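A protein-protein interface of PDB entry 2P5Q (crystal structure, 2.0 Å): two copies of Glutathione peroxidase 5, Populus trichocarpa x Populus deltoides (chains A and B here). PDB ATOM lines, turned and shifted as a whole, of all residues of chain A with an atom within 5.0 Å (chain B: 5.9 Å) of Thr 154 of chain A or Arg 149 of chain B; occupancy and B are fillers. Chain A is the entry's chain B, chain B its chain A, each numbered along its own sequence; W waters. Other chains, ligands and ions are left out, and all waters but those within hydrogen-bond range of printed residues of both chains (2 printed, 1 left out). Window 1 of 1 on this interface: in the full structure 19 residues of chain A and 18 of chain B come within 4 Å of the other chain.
The side-chain hydroxyl (OH) of Tyr 151 of chain A is in hydrogen-bond range of the side-chain carboxylate (OD1) of Asp 129 of chain B (2.8 Å).
OH of Tyr 151 of chain A lies within hydrogen-bond range of NE2 of Gln 132 of chain B, 2.8 Å away.
NE of Arg 149 of chain B is in hydrogen-bond range of OH of Tyr 151 of chain A (2.9 Å).
The side-chain carboxylate of Asp 162 of chain B is in hydrogen-bond range of the side-chain hydroxyl of Ser 158 of chain A.
Among the printed residues, pairs that only touch across the chains: Thr 153 of chain A with Phe 127 of chain B (3.1 Å), Tyr 151 of chain A with Tyr 151 of chain B (3.2 Å), Tyr 151 of chain A with Ile 126 of chain B (3.4 Å), Thr 153 of chain A with Asp 148 of chain B (3.6 Å), Pro 152 of chain A with Ile 126 of chain B (3.8 Å), Tyr 151 of chain A with Phe 127 of chain B (3.8 Å), Thr 154 of chain A with Arg 149 of chain B (3.9 Å) and Thr 154 of chain A with Tyr 150 of chain B (3.99 Å).
Tyr 151 of chain A touches its own counterpart, Tyr 151 of chain B.
Positions printed for both chains: 137, 150 and 151.
Of the 12 pairs that touch across the chains among the printed residues, 1 has its exchanged pair printed and touching as well.
Water W2 lies within hydrogen-bond range of the side-chain hydroxyl of Thr 154 of chain A, the backbone carbonyl oxygen of Arg 149 of chain B and the backbone NH of Tyr 151 of chain A.
Water W1 lies within hydrogen-bond range of OG1 of Thr 153 of chain A (2.7 Å), OG1 of Thr 154 of chain A (2.8 Å) and N of Arg 149 of chain B (3.2 Å).
Of the 11 printed residues of chain A, 5 touch a printed residue of chain B.
Hydrophobic or aromatic side chains of chain A that line the printed part of chain B: Tyr 151 and Pro 152.
Hydrophobic or aromatic side chains of chain B that line the printed part of chain A: Ile 126, Phe 127, Tyr 150 and Tyr 151.
Of the printed residues of chain B, Thr 154 of chain A touches Arg 149 (3.9 Å) and Tyr 150 (3.99 Å).
Of the printed residues of chain B, Ser 158 of chain A touches Asp 162 (2.8 Å).
Of the printed residues of chain A, Phe 127 of chain B touches Tyr 151 and Thr 153.
Of the printed residues of chain A, Asp 148 of chain B touches Thr 153 (3.6 Å).
Of the printed residues of chain A, Tyr 150 of chain B touches Thr 154.
Of the printed residues of chain A, Tyr 151 of chain B touches Tyr 151 (3.2 Å).
The nearest printed residue of chain B that does not touch Thr 154 of chain A is Asp 148 of chain B (4.3 Å).
The nearest residue of chain A that does not touch Arg 149 of chain B is Thr 153 of chain A (4.7 Å).
The nearest printed residue of chain A that does not touch Asp 148 of chain B is Thr 154 of chain A (4.3 Å).
The guanidinium group (NH1) of Arg 149 of chain B lies within hydrogen-bond range of the backbone carbonyl oxygen (O) of Asp 129 of chain B (2.8 Å).
The side-chain amide oxygen (OE1) of Gln 132 of chain B lies within hydrogen-bond range of the guanidinium group (NH2) of Arg 149 of chain B (3.0 Å).
N of Tyr 150 of chain B lies within hydrogen-bond range of O of Lys 137 of chain B, at 2.8 Å.
The side-chain hydroxyl (OH) of Tyr 150 of chain B lies within hydrogen-bond range of the side-chain carboxylate (OD2) of Asp 162 of chain B.
The side-chain amino group (NZ) of Lys 137 of chain A lies within hydrogen-bond range of the backbone carbonyl oxygen (O) of Pro 152 of chain A, 3.0 Å away.
NZ of Lys 137 of chain A is in hydrogen-bond range of O of Thr 154 of chain A, at 2.7 Å.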
ATOM      1  N   ASN A  50      14.260 -15.142  36.877  1.00  0.00           N
ATOM      2  CA  ASN A  50      14.039 -14.404  35.643  1.00  0.00           C
ATOM      3  C   ASN A  50      14.331 -12.916  35.784  1.00  0.00           C
ATOM      4  O   ASN A  50      15.000 -12.337  34.930  1.00  0.00           O
ATOM      5  CB  ASN A  50      12.619 -14.637  35.134  1.00  0.00           C
ATOM      6  CG  ASN A  50      12.521 -15.874  34.262  1.00  0.00           C
ATOM      7  OD1 ASN A  50      12.717 -15.810  33.049  1.00  0.00           O
ATOM      8  ND2 ASN A  50      12.244 -17.011  34.882  1.00  0.00           N
ATOM      9  N   LYS A 137       9.881 -15.762  26.230  1.00  0.00           N
ATOM     10  CA  LYS A 137      10.707 -14.676  25.721  1.00  0.00           C
ATOM     11  C   LYS A 137      10.721 -14.593  24.206  1.00  0.00           C
ATOM     12  O   LYS A 137      10.641 -15.608  23.510  1.00  0.00           O
ATOM     13  CB  LYS A 137      12.162 -14.822  26.194  1.00  0.00           C
ATOM     14  CG  LYS A 137      12.392 -14.724  27.693  1.00  0.00           C
ATOM     15  CD  LYS A 137      12.246 -16.063  28.393  1.00  0.00           C
ATOM     16  CE  LYS A 137      12.715 -15.955  29.837  1.00  0.00           C
ATOM     17  NZ  LYS A 137      12.407 -17.165  30.640  1.00  0.00           N
ATOM     18  N   TYR A 150      11.527 -18.203  22.915  1.00  0.00           N
ATOM     19  CA  TYR A 150      12.020 -19.172  23.888  1.00  0.00           C
ATOM     20  C   TYR A 150      10.940 -19.592  24.872  1.00  0.00           C
ATOM     21  O   TYR A 150      10.099 -18.784  25.273  1.00  0.00           O
ATOM     22  CB  TYR A 150      13.194 -18.570  24.665  1.00  0.00           C
ATOM     23  CG  TYR A 150      14.276 -18.005  23.782  1.00  0.00           C
ATOM     24  CD1 TYR A 150      15.387 -18.769  23.427  1.00  0.00           C
ATOM     25  CD2 TYR A 150      14.179 -16.706  23.280  1.00  0.00           C
ATOM     26  CE1 TYR A 150      16.378 -18.252  22.589  1.00  0.00           C
ATOM     27  CE2 TYR A 150      15.161 -16.179  22.441  1.00  0.00           C
ATOM     28  CZ  TYR A 150      16.257 -16.956  22.099  1.00  0.00           C
ATOM     29  OH  TYR A 150      17.227 -16.437  21.268  1.00  0.00           O
ATOM     30  N   TYR A 151      10.971 -20.864  25.259  1.00  0.00           N
ATOM     31  CA  TYR A 151      10.012 -21.386  26.221  1.00  0.00           C
ATOM     32  C   TYR A 151      10.243 -20.721  27.572  1.00  0.00           C
ATOM     33  O   TYR A 151      11.348 -20.263  27.862  1.00  0.00           O
ATOM     34  CB  TYR A 151      10.152 -22.909  26.350  1.00  0.00           C
ATOM     35  CG  TYR A 151       9.402 -23.657  25.277  1.00  0.00           C
ATOM     36  CD1 TYR A 151       9.884 -23.714  23.969  1.00  0.00           C
ATOM     37  CD2 TYR A 151       8.161 -24.239  25.550  1.00  0.00           C
ATOM     38  CE1 TYR A 151       9.145 -24.328  22.956  1.00  0.00           C
ATOM     39  CE2 TYR A 151       7.417 -24.851  24.547  1.00  0.00           C
ATOM     40  CZ  TYR A 151       7.912 -24.889  23.254  1.00  0.00           C
ATOM     41  OH  TYR A 151       7.158 -25.460  22.257  1.00  0.00           O
ATOM     42  N   PRO A 152       9.196 -20.648  28.411  1.00  0.00           N
ATOM     43  CA  PRO A 152       9.271 -20.032  29.741  1.00  0.00           C
ATOM     44  C   PRO A 152      10.445 -20.552  30.570  1.00  0.00           C
ATOM     45  O   PRO A 152      11.081 -19.803  31.314  1.00  0.00           O
ATOM     46  CB  PRO A 152       7.928 -20.404  30.365  1.00  0.00           C
ATOM     47  CG  PRO A 152       7.010 -20.437  29.180  1.00  0.00           C
ATOM     48  CD  PRO A 152       7.841 -21.168  28.147  1.00  0.00           C
ATOM     49  N   THR A 153      10.715 -21.843  30.424  1.00  0.00           N
ATOM     50  CA  THR A 153      11.780 -22.529  31.144  1.00  0.00           C
ATOM     51  C   THR A 153      13.205 -22.138  30.758  1.00  0.00           C
ATOM     52  O   THR A 153      14.148 -22.488  31.453  1.00  0.00           O
ATOM     53  CB  THR A 153      11.624 -24.042  30.979  1.00  0.00           C
ATOM     54  OG1 THR A 153      11.351 -24.335  29.605  1.00  0.00           O
ATOM     55  CG2 THR A 153      10.472 -24.557  31.842  1.00  0.00           C
ATOM     56  N   THR A 154      13.369 -21.422  29.653  1.00  0.00           N
ATOM     57  CA  THR A 154      14.700 -20.985  29.238  1.00  0.00           C
ATOM     58  C   THR A 154      15.005 -19.678  29.981  1.00  0.00           C
ATOM     59  O   THR A 154      14.448 -18.633  29.642  1.00  0.00           O
ATOM     60  CB  THR A 154      14.747 -20.738  27.716  1.00  0.00           C
ATOM     61  OG1 THR A 154      14.481 -21.969  27.031  1.00  0.00           O
ATOM     62  CG2 THR A 154      16.121 -20.204  27.286  1.00  0.00           C
ATOM     63  N   SER A 155      15.878 -19.731  30.989  1.00  0.00           N
ATOM     64  CA  SER A 155      16.191 -18.528  31.757  1.00  0.00           C
ATOM     65  C   SER A 155      16.862 -17.473  30.880  1.00  0.00           C
ATOM     66  O   SER A 155      17.511 -17.797  29.885  1.00  0.00           O
ATOM     67  CB  SER A 155      17.063 -18.861  32.979  1.00  0.00           C
ATOM     68  OG  SER A 155      18.432 -18.963  32.647  1.00  0.00           O
ATOM     69  N   PRO A 156      16.699 -16.188  31.239  1.00  0.00           N
ATOM     70  CA  PRO A 156      17.272 -15.063  30.491  1.00  0.00           C
ATOM     71  C   PRO A 156      18.736 -15.204  30.078  1.00  0.00           C
ATOM     72  O   PRO A 156      19.094 -14.850  28.960  1.00  0.00           O
ATOM     73  CB  PRO A 156      17.030 -13.877  31.421  1.00  0.00           C
ATOM     74  CG  PRO A 156      15.719 -14.249  32.069  1.00  0.00           C
ATOM     75  CD  PRO A 156      15.936 -15.705  32.406  1.00  0.00           C
ATOM     76  N   SER A 158      20.271 -17.712  29.172  1.00  0.00           N
ATOM     77  CA  SER A 158      20.416 -18.638  28.053  1.00  0.00           C
ATOM     78  C   SER A 158      20.256 -17.936  26.705  1.00  0.00           C
ATOM     79  O   SER A 158      20.604 -18.494  25.667  1.00  0.00           O
ATOM     80  CB  SER A 158      19.395 -19.774  28.157  1.00  0.00           C
ATOM     81  OG  SER A 158      19.705 -20.640  29.229  1.00  0.00           O
ATOM     82  N   LEU A 159      19.728 -16.715  26.724  1.00  0.00           N
ATOM     83  CA  LEU A 159      19.519 -15.948  25.495  1.00  0.00           C
ATOM     84  C   LEU A 159      20.696 -15.047  25.146  1.00  0.00           C
ATOM     85  O   LEU A 159      20.713 -14.423  24.089  1.00  0.00           O
ATOM     86  CB  LEU A 159      18.266 -15.070  25.615  1.00  0.00           C
ATOM     87  CG  LEU A 159      16.869 -15.690  25.504  1.00  0.00           C
ATOM     88  CD1 LEU A 159      16.636 -16.704  26.610  1.00  0.00           C
ATOM     89  CD2 LEU A 159      15.837 -14.566  25.585  1.00  0.00           C
ATOM     90  N   LYS B 120       7.035 -34.093  25.502  1.00  0.00           N
ATOM     91  CA  LYS B 120       5.995 -33.068  25.540  1.00  0.00           C
ATOM     92  C   LYS B 120       5.310 -32.920  26.896  1.00  0.00           C
ATOM     93  O   LYS B 120       4.668 -31.904  27.162  1.00  0.00           O
ATOM     94  CB  LYS B 120       4.944 -33.339  24.457  1.00  0.00           C
ATOM     95  CG  LYS B 120       5.458 -33.143  23.041  1.00  0.00           C
ATOM     96  CD  LYS B 120       4.382 -33.457  22.008  1.00  0.00           C
ATOM     97  CE  LYS B 120       4.907 -33.265  20.592  1.00  0.00           C
ATOM     98  NZ  LYS B 120       3.897 -33.648  19.564  1.00  0.00           N
ATOM     99  N   ILE B 126       4.397 -27.615  29.957  1.00  0.00           N
ATOM    100  CA  ILE B 126       4.831 -26.418  29.242  1.00  0.00           C
ATOM    101  C   ILE B 126       5.339 -26.811  27.852  1.00  0.00           C
ATOM    102  O   ILE B 126       5.224 -26.040  26.901  1.00  0.00           O
ATOM    103  CB  ILE B 126       5.968 -25.685  30.008  1.00  0.00           C
ATOM    104  CG1 ILE B 126       5.420 -25.079  31.302  1.00  0.00           C
ATOM    105  CG2 ILE B 126       6.595 -24.601  29.127  1.00  0.00           C
ATOM    106  CD1 ILE B 126       4.322 -24.072  31.090  1.00  0.00           C
ATOM    107  N   PHE B 127       5.890 -28.018  27.736  1.00  0.00           N
ATOM    108  CA  PHE B 127       6.418 -28.489  26.455  1.00  0.00           C
ATOM    109  C   PHE B 127       5.374 -29.250  25.632  1.00  0.00           C
ATOM    110  O   PHE B 127       5.724 -30.007  24.731  1.00  0.00           O
ATOM    111  CB  PHE B 127       7.637 -29.401  26.675  1.00  0.00           C
ATOM    112  CG  PHE B 127       8.756 -28.768  27.475  1.00  0.00           C
ATOM    113  CD1 PHE B 127       8.906 -27.385  27.535  1.00  0.00           C
ATOM    114  CD2 PHE B 127       9.681 -29.570  28.144  1.00  0.00           C
ATOM    115  CE1 PHE B 127       9.961 -26.807  28.251  1.00  0.00           C
ATOM    116  CE2 PHE B 127      10.739 -29.006  28.862  1.00  0.00           C
ATOM    117  CZ  PHE B 127      10.880 -27.621  28.916  1.00  0.00           C
ATOM    118  N   GLY B 128       4.095 -29.035  25.932  1.00  0.00           N
ATOM    119  CA  GLY B 128       3.035 -29.737  25.221  1.00  0.00           C
ATOM    120  C   GLY B 128       2.807 -29.436  23.744  1.00  0.00           C
ATOM    121  O   GLY B 128       2.223 -30.256  23.036  1.00  0.00           O
ATOM    122  N   ASP B 129       3.263 -28.281  23.270  1.00  0.00           N
ATOM    123  CA  ASP B 129       3.071 -27.889  21.870  1.00  0.00           C
ATOM    124  C   ASP B 129       3.576 -28.914  20.864  1.00  0.00           C
ATOM    125  O   ASP B 129       4.529 -29.649  21.133  1.00  0.00           O
ATOM    126  CB  ASP B 129       3.800 -26.577  21.563  1.00  0.00           C
ATOM    127  CG  ASP B 129       3.520 -25.497  22.575  1.00  0.00           C
ATOM    128  OD1 ASP B 129       4.497 -24.888  23.056  1.00  0.00           O
ATOM    129  OD2 ASP B 129       2.335 -25.246  22.881  1.00  0.00           O
ATOM    130  N   ASP B 130       2.940 -28.947  19.695  1.00  0.00           N
ATOM    131  CA  ASP B 130       3.376 -29.833  18.624  1.00  0.00           C
ATOM    132  C   ASP B 130       4.757 -29.323  18.233  1.00  0.00           C
ATOM    133  O   ASP B 130       5.040 -28.132  18.376  1.00  0.00           O
ATOM    134  CB  ASP B 130       2.484 -29.699  17.385  1.00  0.00           C
ATOM    135  CG  ASP B 130       1.256 -30.588  17.430  1.00  0.00           C
ATOM    136  OD1 ASP B 130       0.645 -30.768  16.357  1.00  0.00           O
ATOM    137  OD2 ASP B 130       0.894 -31.097  18.512  1.00  0.00           O
ATOM    138  N   ILE B 131       5.616 -30.211  17.745  1.00  0.00           N
ATOM    139  CA  ILE B 131       6.930 -29.781  17.294  1.00  0.00           C
ATOM    140  C   ILE B 131       6.597 -28.811  16.156  1.00  0.00           C
ATOM    141  O   ILE B 131       5.868 -29.168  15.230  1.00  0.00           O
ATOM    142  CB  ILE B 131       7.751 -30.976  16.770  1.00  0.00           C
ATOM    143  CG1 ILE B 131       7.926 -32.003  17.895  1.00  0.00           C
ATOM    144  CG2 ILE B 131       9.102 -30.505  16.241  1.00  0.00           C
ATOM    145  CD1 ILE B 131       8.501 -31.435  19.186  1.00  0.00           C
ATOM    146  N   GLN B 132       7.112 -27.588  16.243  1.00  0.00           N
ATOM    147  CA  GLN B 132       6.825 -26.544  15.258  1.00  0.00           C
ATOM    148  C   GLN B 132       7.376 -26.736  13.847  1.00  0.00           C
ATOM    149  O   GLN B 132       6.729 -26.361  12.861  1.00  0.00           O
ATOM    150  CB  GLN B 132       7.311 -25.189  15.780  1.00  0.00           C
ATOM    151  CG  GLN B 132       6.667 -24.722  17.079  1.00  0.00           C
ATOM    152  CD  GLN B 132       7.265 -25.360  18.326  1.00  0.00           C
ATOM    153  OE1 GLN B 132       8.228 -26.125  18.254  1.00  0.00           O
ATOM    154  NE2 GLN B 132       6.693 -25.036  19.481  1.00  0.00           N
ATOM    155  N   ALA B 136      13.717 -28.827  16.166  1.00  0.00           N
ATOM    156  CA  ALA B 136      13.300 -28.348  17.472  1.00  0.00           C
ATOM    157  C   ALA B 136      14.288 -29.101  18.364  1.00  0.00           C
ATOM    158  O   ALA B 136      14.795 -30.149  17.964  1.00  0.00           O
ATOM    159  CB  ALA B 136      11.874 -28.796  17.778  1.00  0.00           C
ATOM    160  N   LYS B 137      14.581 -28.577  19.549  1.00  0.00           N
ATOM    161  CA  LYS B 137      15.518 -29.256  20.443  1.00  0.00           C
ATOM    162  C   LYS B 137      14.972 -29.427  21.853  1.00  0.00           C
ATOM    163  O   LYS B 137      14.184 -28.613  22.332  1.00  0.00           O
ATOM    164  CB  LYS B 137      16.848 -28.493  20.541  1.00  0.00           C
ATOM    165  CG  LYS B 137      17.650 -28.376  19.248  1.00  0.00           C
ATOM    166  CD  LYS B 137      17.249 -27.149  18.442  1.00  0.00           C
ATOM    167  CE  LYS B 137      18.190 -26.940  17.257  1.00  0.00           C
ATOM    168  NZ  LYS B 137      17.748 -25.823  16.368  1.00  0.00           N
ATOM    169  N   PHE B 138      15.415 -30.495  22.505  1.00  0.00           N
ATOM    170  CA  PHE B 138      15.049 -30.809  23.880  1.00  0.00           C
ATOM    171  C   PHE B 138      16.341 -31.190  24.600  1.00  0.00           C
ATOM    172  O   PHE B 138      17.244 -31.772  23.996  1.00  0.00           O
ATOM    173  CB  PHE B 138      14.118 -32.028  23.949  1.00  0.00           C
ATOM    174  CG  PHE B 138      12.689 -31.746  23.583  1.00  0.00           C
ATOM    175  CD1 PHE B 138      11.777 -31.341  24.554  1.00  0.00           C
ATOM    176  CD2 PHE B 138      12.246 -31.930  22.278  1.00  0.00           C
ATOM    177  CE1 PHE B 138      10.440 -31.131  24.230  1.00  0.00           C
ATOM    178  CE2 PHE B 138      10.914 -31.721  21.941  1.00  0.00           C
ATOM    179  CZ  PHE B 138      10.005 -31.321  22.924  1.00  0.00           C
ATOM    180  N   LEU B 139      16.431 -30.852  25.880  1.00  0.00           N
ATOM    181  CA  LEU B 139      17.579 -31.242  26.691  1.00  0.00           C
ATOM    182  C   LEU B 139      17.015 -32.069  27.839  1.00  0.00           C
ATOM    183  O   LEU B 139      16.018 -31.685  28.457  1.00  0.00           O
ATOM    184  CB  LEU B 139      18.325 -30.027  27.253  1.00  0.00           C
ATOM    185  CG  LEU B 139      19.269 -29.284  26.302  1.00  0.00           C
ATOM    186  CD1 LEU B 139      19.800 -28.036  26.992  1.00  0.00           C
ATOM    187  CD2 LEU B 139      20.421 -30.202  25.878  1.00  0.00           C
ATOM    188  N   VAL B 146      13.193 -34.315  31.243  1.00  0.00           N
ATOM    189  CA  VAL B 146      13.326 -33.258  30.244  1.00  0.00           C
ATOM    190  C   VAL B 146      13.268 -31.907  30.965  1.00  0.00           C
ATOM    191  O   VAL B 146      12.321 -31.618  31.697  1.00  0.00           O
ATOM    192  CB  VAL B 146      12.203 -33.358  29.177  1.00  0.00           C
ATOM    193  CG1 VAL B 146      10.857 -33.184  29.823  1.00  0.00           C
ATOM    194  CG2 VAL B 146      12.421 -32.323  28.074  1.00  0.00           C
ATOM    195  N   VAL B 147      14.290 -31.082  30.762  1.00  0.00           N
ATOM    196  CA  VAL B 147      14.356 -29.791  31.437  1.00  0.00           C
ATOM    197  C   VAL B 147      14.261 -28.557  30.539  1.00  0.00           C
ATOM    198  O   VAL B 147      13.896 -27.475  31.001  1.00  0.00           O
ATOM    199  CB  VAL B 147      15.655 -29.690  32.261  1.00  0.00           C
ATOM    200  CG1 VAL B 147      15.646 -30.733  33.368  1.00  0.00           C
ATOM    201  CG2 VAL B 147      16.867 -29.909  31.358  1.00  0.00           C
ATOM    202  N   ASP B 148      14.588 -28.714  29.263  1.00  0.00           N
ATOM    203  CA  ASP B 148      14.549 -27.592  28.333  1.00  0.00           C
ATOM    204  C   ASP B 148      14.041 -27.962  26.944  1.00  0.00           C
ATOM    205  O   ASP B 148      14.263 -29.073  26.465  1.00  0.00           O
ATOM    206  CB  ASP B 148      15.949 -26.984  28.195  1.00  0.00           C
ATOM    207  CG  ASP B 148      16.373 -26.209  29.423  1.00  0.00           C
ATOM    208  OD1 ASP B 148      15.784 -25.138  29.662  1.00  0.00           O
ATOM    209  OD2 ASP B 148      17.286 -26.667  30.149  1.00  0.00           O
ATOM    210  N   ARG B 149      13.350 -27.016  26.312  1.00  0.00           N
ATOM    211  CA  ARG B 149      12.847 -27.187  24.953  1.00  0.00           C
ATOM    212  C   ARG B 149      13.128 -25.891  24.203  1.00  0.00           C
ATOM    213  O   ARG B 149      13.008 -24.801  24.764  1.00  0.00           O
ATOM    214  CB  ARG B 149      11.343 -27.486  24.926  1.00  0.00           C
ATOM    215  CG  ARG B 149      10.806 -27.558  23.493  1.00  0.00           C
ATOM    216  CD  ARG B 149       9.370 -28.054  23.395  1.00  0.00           C
ATOM    217  NE  ARG B 149       8.847 -27.865  22.043  1.00  0.00           N
ATOM    218  CZ  ARG B 149       7.667 -28.309  21.623  1.00  0.00           C
ATOM    219  NH1 ARG B 149       6.873 -28.983  22.447  1.00  0.00           N
ATOM    220  NH2 ARG B 149       7.269 -28.064  20.384  1.00  0.00           N
ATOM    221  N   TYR B 150      13.510 -26.004  22.935  1.00  0.00           N
ATOM    222  CA  TYR B 150      13.827 -24.821  22.145  1.00  0.00           C
ATOM    223  C   TYR B 150      13.143 -24.820  20.786  1.00  0.00           C
ATOM    224  O   TYR B 150      12.972 -25.869  20.162  1.00  0.00           O
ATOM    225  CB  TYR B 150      15.343 -24.711  21.935  1.00  0.00           C
ATOM    226  CG  TYR B 150      16.159 -24.849  23.203  1.00  0.00           C
ATOM    227  CD1 TYR B 150      16.395 -26.103  23.772  1.00  0.00           C
ATOM    228  CD2 TYR B 150      16.667 -23.725  23.854  1.00  0.00           C
ATOM    229  CE1 TYR B 150      17.114 -26.235  24.958  1.00  0.00           C
ATOM    230  CE2 TYR B 150      17.389 -23.845  25.046  1.00  0.00           C
ATOM    231  CZ  TYR B 150      17.608 -25.102  25.591  1.00  0.00           C
ATOM    232  OH  TYR B 150      18.313 -25.229  26.767  1.00  0.00           O
ATOM    233  N   TYR B 151      12.754 -23.634  20.332  1.00  0.00           N
ATOM    234  CA  TYR B 151      12.121 -23.497  19.027  1.00  0.00           C
ATOM    235  C   TYR B 151      13.143 -23.864  17.957  1.00  0.00           C
ATOM    236  O   TYR B 151      14.351 -23.733  18.169  1.00  0.00           O
ATOM    237  CB  TYR B 151      11.615 -22.066  18.833  1.00  0.00           C
ATOM    238  CG  TYR B 151      10.233 -21.866  19.406  1.00  0.00           C
ATOM    239  CD1 TYR B 151       9.100 -21.991  18.600  1.00  0.00           C
ATOM    240  CD2 TYR B 151      10.049 -21.638  20.770  1.00  0.00           C
ATOM    241  CE1 TYR B 151       7.816 -21.901  19.138  1.00  0.00           C
ATOM    242  CE2 TYR B 151       8.768 -21.551  21.317  1.00  0.00           C
ATOM    243  CZ  TYR B 151       7.658 -21.686  20.493  1.00  0.00           C
ATOM    244  OH  TYR B 151       6.392 -21.625  21.032  1.00  0.00           O
ATOM    245  N   ASP B 162      23.089 -23.827  28.740  1.00  0.00           N
ATOM    246  CA  ASP B 162      22.313 -24.811  29.491  1.00  0.00           C
ATOM    247  C   ASP B 162      23.023 -26.158  29.526  1.00  0.00           C
ATOM    248  O   ASP B 162      22.974 -26.872  30.532  1.00  0.00           O
ATOM    249  CB  ASP B 162      20.919 -24.984  28.883  1.00  0.00           C
ATOM    250  CG  ASP B 162      20.056 -23.746  29.036  1.00  0.00           C
ATOM    251  OD1 ASP B 162      19.918 -23.256  30.177  1.00  0.00           O
ATOM    252  OD2 ASP B 162      19.513 -23.263  28.019  1.00  0.00           O
HETATM  253  O   HOH W   1      13.645 -24.434  28.159  1.00  0.00           O
HETATM  254  O   HOH W   2      13.461 -22.062  24.558  1.00  0.00           O
